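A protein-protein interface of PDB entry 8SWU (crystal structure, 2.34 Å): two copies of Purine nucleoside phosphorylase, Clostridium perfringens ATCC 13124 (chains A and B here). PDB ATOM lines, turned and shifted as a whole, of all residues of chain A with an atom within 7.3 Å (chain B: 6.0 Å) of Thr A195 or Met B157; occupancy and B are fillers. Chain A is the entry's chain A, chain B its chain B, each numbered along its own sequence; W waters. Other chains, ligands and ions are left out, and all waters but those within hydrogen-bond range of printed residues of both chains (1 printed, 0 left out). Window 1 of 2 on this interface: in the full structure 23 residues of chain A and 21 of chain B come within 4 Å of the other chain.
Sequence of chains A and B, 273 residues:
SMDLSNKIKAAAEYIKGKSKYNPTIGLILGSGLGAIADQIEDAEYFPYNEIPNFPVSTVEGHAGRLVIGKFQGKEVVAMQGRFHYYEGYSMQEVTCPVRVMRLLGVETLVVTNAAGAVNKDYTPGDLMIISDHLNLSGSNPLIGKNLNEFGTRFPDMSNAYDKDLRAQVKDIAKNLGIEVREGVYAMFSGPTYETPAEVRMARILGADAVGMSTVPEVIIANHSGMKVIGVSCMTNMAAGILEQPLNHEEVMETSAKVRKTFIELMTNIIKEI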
ATOM      1  N   PHE A 188     -29.466   6.893  -8.495  1.00  0.00           N
ATOM      2  CA  PHE A 188     -29.408   5.789  -7.552  1.00  0.00           C
ATOM      3  C   PHE A 188     -28.176   5.954  -6.671  1.00  0.00           C
ATOM      4  O   PHE A 188     -27.248   6.701  -6.994  1.00  0.00           O
ATOM      5  CB  PHE A 188     -29.374   4.439  -8.277  1.00  0.00           C
ATOM      6  CG  PHE A 188     -30.661   4.090  -8.980  1.00  0.00           C
ATOM      7  CD1 PHE A 188     -31.014   4.713 -10.166  1.00  0.00           C
ATOM      8  CD2 PHE A 188     -31.518   3.137  -8.452  1.00  0.00           C
ATOM      9  CE1 PHE A 188     -32.197   4.392 -10.813  1.00  0.00           C
ATOM     10  CE2 PHE A 188     -32.703   2.812  -9.095  1.00  0.00           C
ATOM     11  CZ  PHE A 188     -33.041   3.441 -10.278  1.00  0.00           C
ATOM     12  N   THR A 192     -23.295  -0.129  -7.259  1.00  0.00           N
ATOM     13  CA  THR A 192     -23.727  -1.127  -8.226  1.00  0.00           C
ATOM     14  C   THR A 192     -24.338  -0.452  -9.446  1.00  0.00           C
ATOM     15  O   THR A 192     -24.984   0.594  -9.339  1.00  0.00           O
ATOM     16  CB  THR A 192     -24.759  -2.071  -7.603  1.00  0.00           C
ATOM     17  OG1 THR A 192     -25.623  -1.328  -6.733  1.00  0.00           O
ATOM     18  CG2 THR A 192     -24.077  -3.177  -6.811  1.00  0.00           C
ATOM     19  N   TYR A 193     -24.123  -1.047 -10.615  1.00  0.00           N
ATOM     20  CA  TYR A 193     -24.932  -0.688 -11.767  1.00  0.00           C
ATOM     21  C   TYR A 193     -26.336  -1.251 -11.587  1.00  0.00           C
ATOM     22  O   TYR A 193     -26.529  -2.315 -10.993  1.00  0.00           O
ATOM     23  CB  TYR A 193     -24.312  -1.217 -13.058  1.00  0.00           C
ATOM     24  CG  TYR A 193     -23.078  -0.467 -13.502  1.00  0.00           C
ATOM     25  CD1 TYR A 193     -23.133   0.890 -13.794  1.00  0.00           C
ATOM     26  CD2 TYR A 193     -21.857  -1.116 -13.632  1.00  0.00           C
ATOM     27  CE1 TYR A 193     -22.004   1.579 -14.201  1.00  0.00           C
ATOM     28  CE2 TYR A 193     -20.725  -0.437 -14.039  1.00  0.00           C
ATOM     29  CZ  TYR A 193     -20.805   0.910 -14.320  1.00  0.00           C
ATOM     30  OH  TYR A 193     -19.681   1.588 -14.724  1.00  0.00           O
ATOM     31  N   GLU A 194     -27.322  -0.521 -12.096  1.00  0.00           N
ATOM     32  CA  GLU A 194     -28.711  -0.918 -11.905  1.00  0.00           C
ATOM     33  C   GLU A 194     -28.976  -2.270 -12.558  1.00  0.00           C
ATOM     34  O   GLU A 194     -28.335  -2.645 -13.541  1.00  0.00           O
ATOM     35  CB  GLU A 194     -29.656   0.136 -12.486  1.00  0.00           C
ATOM     36  CG  GLU A 194     -29.551   1.514 -11.837  1.00  0.00           C
ATOM     37  CD  GLU A 194     -28.290   2.259 -12.237  1.00  0.00           C
ATOM     38  OE1 GLU A 194     -27.841   2.091 -13.392  1.00  0.00           O
ATOM     39  OE2 GLU A 194     -27.741   3.001 -11.394  1.00  0.00           O
ATOM     40  N   THR A 195     -29.915  -3.013 -11.987  1.00  0.00           N
ATOM     41  CA  THR A 195     -30.371  -4.234 -12.629  1.00  0.00           C
ATOM     42  C   THR A 195     -31.284  -3.891 -13.800  1.00  0.00           C
ATOM     43  O   THR A 195     -31.846  -2.793 -13.858  1.00  0.00           O
ATOM     44  CB  THR A 195     -31.110  -5.120 -11.629  1.00  0.00           C
ATOM     45  OG1 THR A 195     -32.359  -4.511 -11.278  1.00  0.00           O
ATOM     46  CG2 THR A 195     -30.274  -5.318 -10.373  1.00  0.00           C
ATOM     47  N   PRO A 196     -31.423  -4.800 -14.771  1.00  0.00           N
ATOM     48  CA  PRO A 196     -32.408  -4.571 -15.843  1.00  0.00           C
ATOM     49  C   PRO A 196     -33.799  -4.240 -15.324  1.00  0.00           C
ATOM     50  O   PRO A 196     -34.490  -3.400 -15.912  1.00  0.00           O
ATOM     51  CB  PRO A 196     -32.386  -5.894 -16.619  1.00  0.00           C
ATOM     52  CG  PRO A 196     -31.003  -6.413 -16.416  1.00  0.00           C
ATOM     53  CD  PRO A 196     -30.584  -5.985 -15.031  1.00  0.00           C
ATOM     54  N   ALA A 197     -34.222  -4.869 -14.224  1.00  0.00           N
ATOM     55  CA  ALA A 197     -35.534  -4.562 -13.660  1.00  0.00           C
ATOM     56  C   ALA A 197     -35.573  -3.155 -13.079  1.00  0.00           C
ATOM     57  O   ALA A 197     -36.580  -2.449 -13.209  1.00  0.00           O
ATOM     58  CB  ALA A 197     -35.905  -5.594 -12.595  1.00  0.00           C
ATOM     59  N   GLU A 198     -34.488  -2.727 -12.429  1.00  0.00           N
ATOM     60  CA  GLU A 198     -34.454  -1.381 -11.868  1.00  0.00           C
ATOM     61  C   GLU A 198     -34.423  -0.320 -12.962  1.00  0.00           C
ATOM     62  O   GLU A 198     -34.932   0.789 -12.762  1.00  0.00           O
ATOM     63  CB  GLU A 198     -33.252  -1.234 -10.934  1.00  0.00           C
ATOM     64  CG  GLU A 198     -33.522  -1.720  -9.516  1.00  0.00           C
ATOM     65  CD  GLU A 198     -32.253  -2.083  -8.767  1.00  0.00           C
ATOM     66  OE1 GLU A 198     -31.168  -2.054  -9.381  1.00  0.00           O
ATOM     67  OE2 GLU A 198     -32.343  -2.400  -7.562  1.00  0.00           O
ATOM     68  N   VAL A 199     -33.841  -0.641 -14.120  1.00  0.00           N
ATOM     69  CA  VAL A 199     -33.840   0.298 -15.236  1.00  0.00           C
ATOM     70  C   VAL A 199     -35.241   0.440 -15.815  1.00  0.00           C
ATOM     71  O   VAL A 199     -35.682   1.549 -16.146  1.00  0.00           O
ATOM     72  CB  VAL A 199     -32.826  -0.149 -16.303  1.00  0.00           C
ATOM     73  CG1 VAL A 199     -32.980   0.687 -17.563  1.00  0.00           C
ATOM     74  CG2 VAL A 199     -31.413  -0.051 -15.758  1.00  0.00           C
ATOM     75  N   ARG A 200     -35.965  -0.674 -15.943  1.00  0.00           N
ATOM     76  CA  ARG A 200     -37.343  -0.606 -16.420  1.00  0.00           C
ATOM     77  C   ARG A 200     -38.234   0.125 -15.426  1.00  0.00           C
ATOM     78  O   ARG A 200     -39.156   0.845 -15.826  1.00  0.00           O
ATOM     79  CB  ARG A 200     -37.874  -2.011 -16.692  1.00  0.00           C
ATOM     80  CG  ARG A 200     -37.234  -2.686 -17.896  1.00  0.00           C
ATOM     81  CD  ARG A 200     -37.963  -3.966 -18.252  1.00  0.00           C
ATOM     82  NE  ARG A 200     -38.207  -4.798 -17.079  1.00  0.00           N
ATOM     83  CZ  ARG A 200     -37.443  -5.817 -16.711  1.00  0.00           C
ATOM     84  NH1 ARG A 200     -36.369  -6.161 -17.403  1.00  0.00           N
ATOM     85  NH2 ARG A 200     -37.768  -6.512 -15.625  1.00  0.00           N
ATOM     86  N   MET A 201     -37.976  -0.041 -14.125  1.00  0.00           N
ATOM     87  CA  MET A 201     -38.697   0.753 -13.135  1.00  0.00           C
ATOM     88  C   MET A 201     -38.327   2.226 -13.248  1.00  0.00           C
ATOM     89  O   MET A 201     -39.193   3.100 -13.120  1.00  0.00           O
ATOM     90  CB  MET A 201     -38.422   0.227 -11.722  1.00  0.00           C
ATOM     91  CG  MET A 201     -38.366   1.305 -10.652  1.00  0.00           C
ATOM     92  SD  MET A 201     -37.875   0.706  -9.023  1.00  0.00           S
ATOM     93  CE  MET A 201     -36.179   1.279  -8.960  1.00  0.00           C
ATOM     94  N   ALA A 238     -28.489   2.189 -20.607  1.00  0.00           N
ATOM     95  CA  ALA A 238     -28.696   1.656 -19.270  1.00  0.00           C
ATOM     96  C   ALA A 238     -28.811   0.133 -19.307  1.00  0.00           C
ATOM     97  O   ALA A 238     -29.089  -0.472 -20.345  1.00  0.00           O
ATOM     98  CB  ALA A 238     -29.943   2.275 -18.640  1.00  0.00           C
ATOM     99  N   ALA A 239     -28.585  -0.483 -18.148  1.00  0.00           N
ATOM    100  CA  ALA A 239     -28.475  -1.935 -18.075  1.00  0.00           C
ATOM    101  C   ALA A 239     -29.758  -2.615 -18.532  1.00  0.00           C
ATOM    102  O   ALA A 239     -30.866  -2.167 -18.226  1.00  0.00           O
ATOM    103  CB  ALA A 239     -28.136  -2.367 -16.648  1.00  0.00           C
ATOM    104  N   GLY A 240     -29.600  -3.710 -19.270  1.00  0.00           N
ATOM    105  CA  GLY A 240     -30.716  -4.483 -19.756  1.00  0.00           C
ATOM    106  C   GLY A 240     -31.212  -4.099 -21.132  1.00  0.00           C
ATOM    107  O   GLY A 240     -31.924  -4.892 -21.759  1.00  0.00           O
ATOM    108  N   PRO A 245     -22.631  -6.598 -20.609  1.00  0.00           N
ATOM    109  CA  PRO A 245     -22.385  -6.126 -19.245  1.00  0.00           C
ATOM    110  C   PRO A 245     -22.014  -4.654 -19.260  1.00  0.00           C
ATOM    111  O   PRO A 245     -21.485  -4.132 -20.244  1.00  0.00           O
ATOM    112  CB  PRO A 245     -21.215  -6.993 -18.774  1.00  0.00           C
ATOM    113  CG  PRO A 245     -20.492  -7.339 -20.033  1.00  0.00           C
ATOM    114  CD  PRO A 245     -21.552  -7.475 -21.096  1.00  0.00           C
ATOM    115  N   LEU A 246     -22.310  -3.976 -18.157  1.00  0.00           N
ATOM    116  CA  LEU A 246     -21.925  -2.582 -18.005  1.00  0.00           C
ATOM    117  C   LEU A 246     -20.547  -2.500 -17.365  1.00  0.00           C
ATOM    118  O   LEU A 246     -20.259  -3.198 -16.389  1.00  0.00           O
ATOM    119  CB  LEU A 246     -22.953  -1.812 -17.179  1.00  0.00           C
ATOM    120  CG  LEU A 246     -24.048  -1.186 -18.046  1.00  0.00           C
ATOM    121  CD1 LEU A 246     -25.012  -0.348 -17.215  1.00  0.00           C
ATOM    122  CD2 LEU A 246     -23.426  -0.364 -19.164  1.00  0.00           C
ATOM    123  N   ASP B 132     -34.556 -11.471 -11.617  1.00  0.00           N
ATOM    124  CA  ASP B 132     -33.961 -10.170 -11.337  1.00  0.00           C
ATOM    125  C   ASP B 132     -34.578  -9.655 -10.045  1.00  0.00           C
ATOM    126  O   ASP B 132     -35.512 -10.252  -9.506  1.00  0.00           O
ATOM    127  CB  ASP B 132     -34.180  -9.188 -12.492  1.00  0.00           C
ATOM    128  CG  ASP B 132     -33.012  -8.241 -12.680  1.00  0.00           C
ATOM    129  OD1 ASP B 132     -32.004  -8.388 -11.957  1.00  0.00           O
ATOM    130  OD2 ASP B 132     -33.102  -7.350 -13.552  1.00  0.00           O
ATOM    131  N   HIS B 133     -34.048  -8.540  -9.547  1.00  0.00           N
ATOM    132  CA  HIS B 133     -34.559  -7.993  -8.300  1.00  0.00           C
ATOM    133  C   HIS B 133     -34.637  -6.474  -8.364  1.00  0.00           C
ATOM    134  O   HIS B 133     -34.024  -5.828  -9.217  1.00  0.00           O
ATOM    135  CB  HIS B 133     -33.724  -8.452  -7.087  1.00  0.00           C
ATOM    136  CG  HIS B 133     -32.357  -7.844  -7.005  1.00  0.00           C
ATOM    137  ND1 HIS B 133     -31.213  -8.609  -6.928  1.00  0.00           N
ATOM    138  CD2 HIS B 133     -31.949  -6.553  -6.947  1.00  0.00           C
ATOM    139  CE1 HIS B 133     -30.159  -7.816  -6.850  1.00  0.00           C
ATOM    140  NE2 HIS B 133     -30.579  -6.563  -6.860  1.00  0.00           N
ATOM    141  N   LEU B 134     -35.422  -5.919  -7.441  1.00  0.00           N
ATOM    142  CA  LEU B 134     -35.528  -4.481  -7.222  1.00  0.00           C
ATOM    143  C   LEU B 134     -35.150  -4.193  -5.776  1.00  0.00           C
ATOM    144  O   LEU B 134     -35.762  -4.742  -4.854  1.00  0.00           O
ATOM    145  CB  LEU B 134     -36.945  -3.975  -7.510  1.00  0.00           C
ATOM    146  CG  LEU B 134     -37.530  -4.175  -8.906  1.00  0.00           C
ATOM    147  CD1 LEU B 134     -39.052  -4.064  -8.870  1.00  0.00           C
ATOM    148  CD2 LEU B 134     -36.941  -3.159  -9.864  1.00  0.00           C
ATOM    149  N   PRO B 155     -19.532  -2.865  -9.901  1.00  0.00           N
ATOM    150  CA  PRO B 155     -19.834  -4.213 -10.389  1.00  0.00           C
ATOM    151  C   PRO B 155     -21.073  -4.224 -11.269  1.00  0.00           C
ATOM    152  O   PRO B 155     -22.019  -3.458 -11.070  1.00  0.00           O
ATOM    153  CB  PRO B 155     -20.058  -5.012  -9.102  1.00  0.00           C
ATOM    154  CG  PRO B 155     -20.563  -3.999  -8.131  1.00  0.00           C
ATOM    155  CD  PRO B 155     -19.899  -2.690  -8.485  1.00  0.00           C
ATOM    156  N   ASP B 156     -21.053  -5.112 -12.259  1.00  0.00           N
ATOM    157  CA  ASP B 156     -22.169  -5.249 -13.181  1.00  0.00           C
ATOM    158  C   ASP B 156     -23.281  -6.074 -12.546  1.00  0.00           C
ATOM    159  O   ASP B 156     -23.022  -7.023 -11.800  1.00  0.00           O
ATOM    160  CB  ASP B 156     -21.704  -5.898 -14.484  1.00  0.00           C
ATOM    161  CG  ASP B 156     -22.853  -6.215 -15.421  1.00  0.00           C
ATOM    162  OD1 ASP B 156     -23.416  -5.271 -16.011  1.00  0.00           O
ATOM    163  OD2 ASP B 156     -23.189  -7.408 -15.568  1.00  0.00           O
ATOM    164  N   MET B 157     -24.529  -5.698 -12.839  1.00  0.00           N
ATOM    165  CA  MET B 157     -25.697  -6.377 -12.290  1.00  0.00           C
ATOM    166  C   MET B 157     -26.656  -6.829 -13.387  1.00  0.00           C
ATOM    167  O   MET B 157     -27.852  -6.991 -13.128  1.00  0.00           O
ATOM    168  CB  MET B 157     -26.432  -5.474 -11.291  1.00  0.00           C
ATOM    169  CG  MET B 157     -25.817  -5.381  -9.891  1.00  0.00           C
ATOM    170  SD  MET B 157     -25.364  -6.962  -9.144  1.00  0.00           S
ATOM    171  CE  MET B 157     -26.757  -7.217  -8.057  1.00  0.00           C
ATOM    172  N   SER B 158     -26.162  -7.032 -14.610  1.00  0.00           N
ATOM    173  CA  SER B 158     -27.006  -7.479 -15.712  1.00  0.00           C
ATOM    174  C   SER B 158     -27.241  -8.984 -15.711  1.00  0.00           C
ATOM    175  O   SER B 158     -28.110  -9.460 -16.449  1.00  0.00           O
ATOM    176  CB  SER B 158     -26.391  -7.056 -17.050  1.00  0.00           C
ATOM    177  OG  SER B 158     -26.316  -5.645 -17.155  1.00  0.00           O
ATOM    178  N   ASN B 159     -26.491  -9.735 -14.911  1.00  0.00           N
ATOM    179  CA  ASN B 159     -26.654 -11.178 -14.771  1.00  0.00           C
ATOM    180  C   ASN B 159     -26.513 -11.543 -13.296  1.00  0.00           C
ATOM    181  O   ASN B 159     -25.737 -12.418 -12.915  1.00  0.00           O
ATOM    182  CB  ASN B 159     -25.642 -11.930 -15.639  1.00  0.00           C
ATOM    183  CG  ASN B 159     -26.026 -13.385 -15.876  1.00  0.00           C
ATOM    184  OD1 ASN B 159     -27.203 -13.719 -16.019  1.00  0.00           O
ATOM    185  ND2 ASN B 159     -25.024 -14.257 -15.923  1.00  0.00           N
ATOM    186  N   ALA B 160     -27.262 -10.834 -12.445  1.00  0.00           N
ATOM    187  CA  ALA B 160     -27.187 -11.066 -11.005  1.00  0.00           C
ATOM    188  C   ALA B 160     -27.654 -12.467 -10.637  1.00  0.00           C
ATOM    189  O   ALA B 160     -27.131 -13.069  -9.692  1.00  0.00           O
ATOM    190  CB  ALA B 160     -28.020 -10.023 -10.260  1.00  0.00           C
ATOM    191  N   VAL B 215     -31.662  -9.641  -1.481  1.00  0.00           N
ATOM    192  CA  VAL B 215     -30.982  -8.646  -2.322  1.00  0.00           C
ATOM    193  C   VAL B 215     -29.608  -8.259  -1.786  1.00  0.00           C
ATOM    194  O   VAL B 215     -28.670  -8.142  -2.589  1.00  0.00           O
ATOM    195  CB  VAL B 215     -31.899  -7.438  -2.557  1.00  0.00           C
ATOM    196  CG1 VAL B 215     -31.116  -6.254  -3.105  1.00  0.00           C
ATOM    197  CG2 VAL B 215     -33.026  -7.813  -3.509  1.00  0.00           C
ATOM    198  N   VAL B 218     -27.064 -11.135  -2.578  1.00  0.00           N
ATOM    199  CA  VAL B 218     -26.908 -11.318  -4.016  1.00  0.00           C
ATOM    200  C   VAL B 218     -25.989 -10.246  -4.591  1.00  0.00           C
ATOM    201  O   VAL B 218     -25.166 -10.520  -5.474  1.00  0.00           O
ATOM    202  CB  VAL B 218     -28.287 -11.323  -4.704  1.00  0.00           C
ATOM    203  CG1 VAL B 218     -28.139 -11.320  -6.217  1.00  0.00           C
ATOM    204  CG2 VAL B 218     -29.091 -12.535  -4.257  1.00  0.00           C
ATOM    205  N   ILE B 219     -26.096  -9.018  -4.084  1.00  0.00           N
ATOM    206  CA  ILE B 219     -25.230  -7.935  -4.544  1.00  0.00           C
ATOM    207  C   ILE B 219     -23.773  -8.250  -4.222  1.00  0.00           C
ATOM    208  O   ILE B 219     -22.884  -8.111  -5.071  1.00  0.00           O
ATOM    209  CB  ILE B 219     -25.670  -6.598  -3.918  1.00  0.00           C
ATOM    210  CG1 ILE B 219     -26.909  -6.052  -4.629  1.00  0.00           C
ATOM    211  CG2 ILE B 219     -24.538  -5.583  -3.955  1.00  0.00           C
ATOM    212  CD1 ILE B 219     -27.595  -4.935  -3.870  1.00  0.00           C
ATOM    213  N   ASN B 222     -22.266 -11.368  -6.242  1.00  0.00           N
ATOM    214  CA  ASN B 222     -21.871 -11.008  -7.599  1.00  0.00           C
ATOM    215  C   ASN B 222     -20.581 -10.197  -7.595  1.00  0.00           C
ATOM    216  O   ASN B 222     -19.679 -10.446  -8.406  1.00  0.00           O
ATOM    217  CB  ASN B 222     -22.989 -10.223  -8.284  1.00  0.00           C
ATOM    218  CG  ASN B 222     -24.002 -11.121  -8.957  1.00  0.00           C
ATOM    219  OD1 ASN B 222     -23.918 -11.379 -10.159  1.00  0.00           O
ATOM    220  ND2 ASN B 222     -24.976 -11.596  -8.188  1.00  0.00           N
ATOM    221  N   HIS B 223     -20.476  -9.223  -6.685  1.00  0.00           N
ATOM    222  CA  HIS B 223     -19.268  -8.407  -6.602  1.00  0.00           C
ATOM    223  C   HIS B 223     -18.051  -9.242  -6.231  1.00  0.00           C
ATOM    224  O   HIS B 223     -16.936  -8.944  -6.674  1.00  0.00           O
ATOM    225  CB  HIS B 223     -19.469  -7.281  -5.588  1.00  0.00           C
ATOM    226  CG  HIS B 223     -18.240  -6.458  -5.346  1.00  0.00           C
ATOM    227  ND1 HIS B 223     -17.400  -6.671  -4.273  1.00  0.00           N
ATOM    228  CD2 HIS B 223     -17.714  -5.414  -6.031  1.00  0.00           C
ATOM    229  CE1 HIS B 223     -16.410  -5.798  -4.311  1.00  0.00           C
ATOM    230  NE2 HIS B 223     -16.577  -5.023  -5.367  1.00  0.00           N
HETATM  231  O   HOH W   1     -25.937  -3.668 -14.511  1.00  0.00           O
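Thr A192 touches Pro B155.
CG2 of Ile B219 touches CG2 of Thr A192 (3.8 Å).
Thr A195 touches Asp B132.
Met B157 touches Thr A195 (O to CA, 3.8 Å).
CD of Pro A196 touches O of Met B157, 3.5 Å away.
Pro A196 touches Ser B158.
O of Ala A197 touches CD2 of Leu B134, at 3.4 Å.
Glu A198 touches Leu B134.
Ala A239 touches Ser B158 (CB to OG, 3.8 Å).
Pro A245 touches Asp B156 (CA to OD1, 3.5 Å).
The side-chain hydroxyl (OG1) of Thr A195 lies within hydrogen-bond range of the backbone NH (N) of Glu A198, at 3.0 Å.
The side-chain hydroxyl (OG) of Ser B158 lies within hydrogen-bond range of the side-chain carboxylate (OD1) of Asp B156.
No position is printed for both chains.
Of chain B, only Asp B132 (3.4 Å), His B133 (3.0 Å) and Met B157 (3.8 Å) come within 4 Å of Thr A195.
Of the printed residues of chain B, Ala A197 touches Asp B132, His B133 and Leu B134.
Val A199 touches none of the printed residues of chain B.
Printed residues of chain A within 4 Å of Asp B132: Thr A195 (3.4 Å), Pro A196 (3.2 Å) and Ala A197 (2.8 Å).
Of chain A, only Tyr A193, Thr A195 and Pro A196 come within 4 Å of Met B157.
Val B215 touches none of the printed residues of chain A.
O of Pro B155 sits at hydrogen-bond distance from N of Tyr A193 (3.2 Å).
The side-chain hydroxyl of Thr A195 sits at hydrogen-bond distance from the backbone carbonyl oxygen of His B133 (3.0 Å).
The backbone NH of Ala A197 sits at hydrogen-bond distance from the side-chain carboxylate of Asp B132 (2.8 Å).
The backbone NH (N) of Leu A246 is in hydrogen-bond range of the side-chain carboxylate (OD1) of Asp B156 (2.7 Å).
The backbone nitrogen of Pro A196 lies close to the side-chain carboxylate of Asp B132 (3.3 Å).
Water W1 lies within hydrogen-bond range of O of Glu A194, N of Met B157, OG of Ser B158 and OD1 of Asp B156.
Printed residues of chain A that touch a printed residue of chain B: Thr A192, Tyr A193, Thr A195, Pro A196, Ala A197, Glu A198, Ala A239, Pro A245 and Leu A246.
Among the printed residues, no Asp or Glu carboxylate lies within 4 Å of a Lys or Arg side-chain nitrogen of the other chain.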
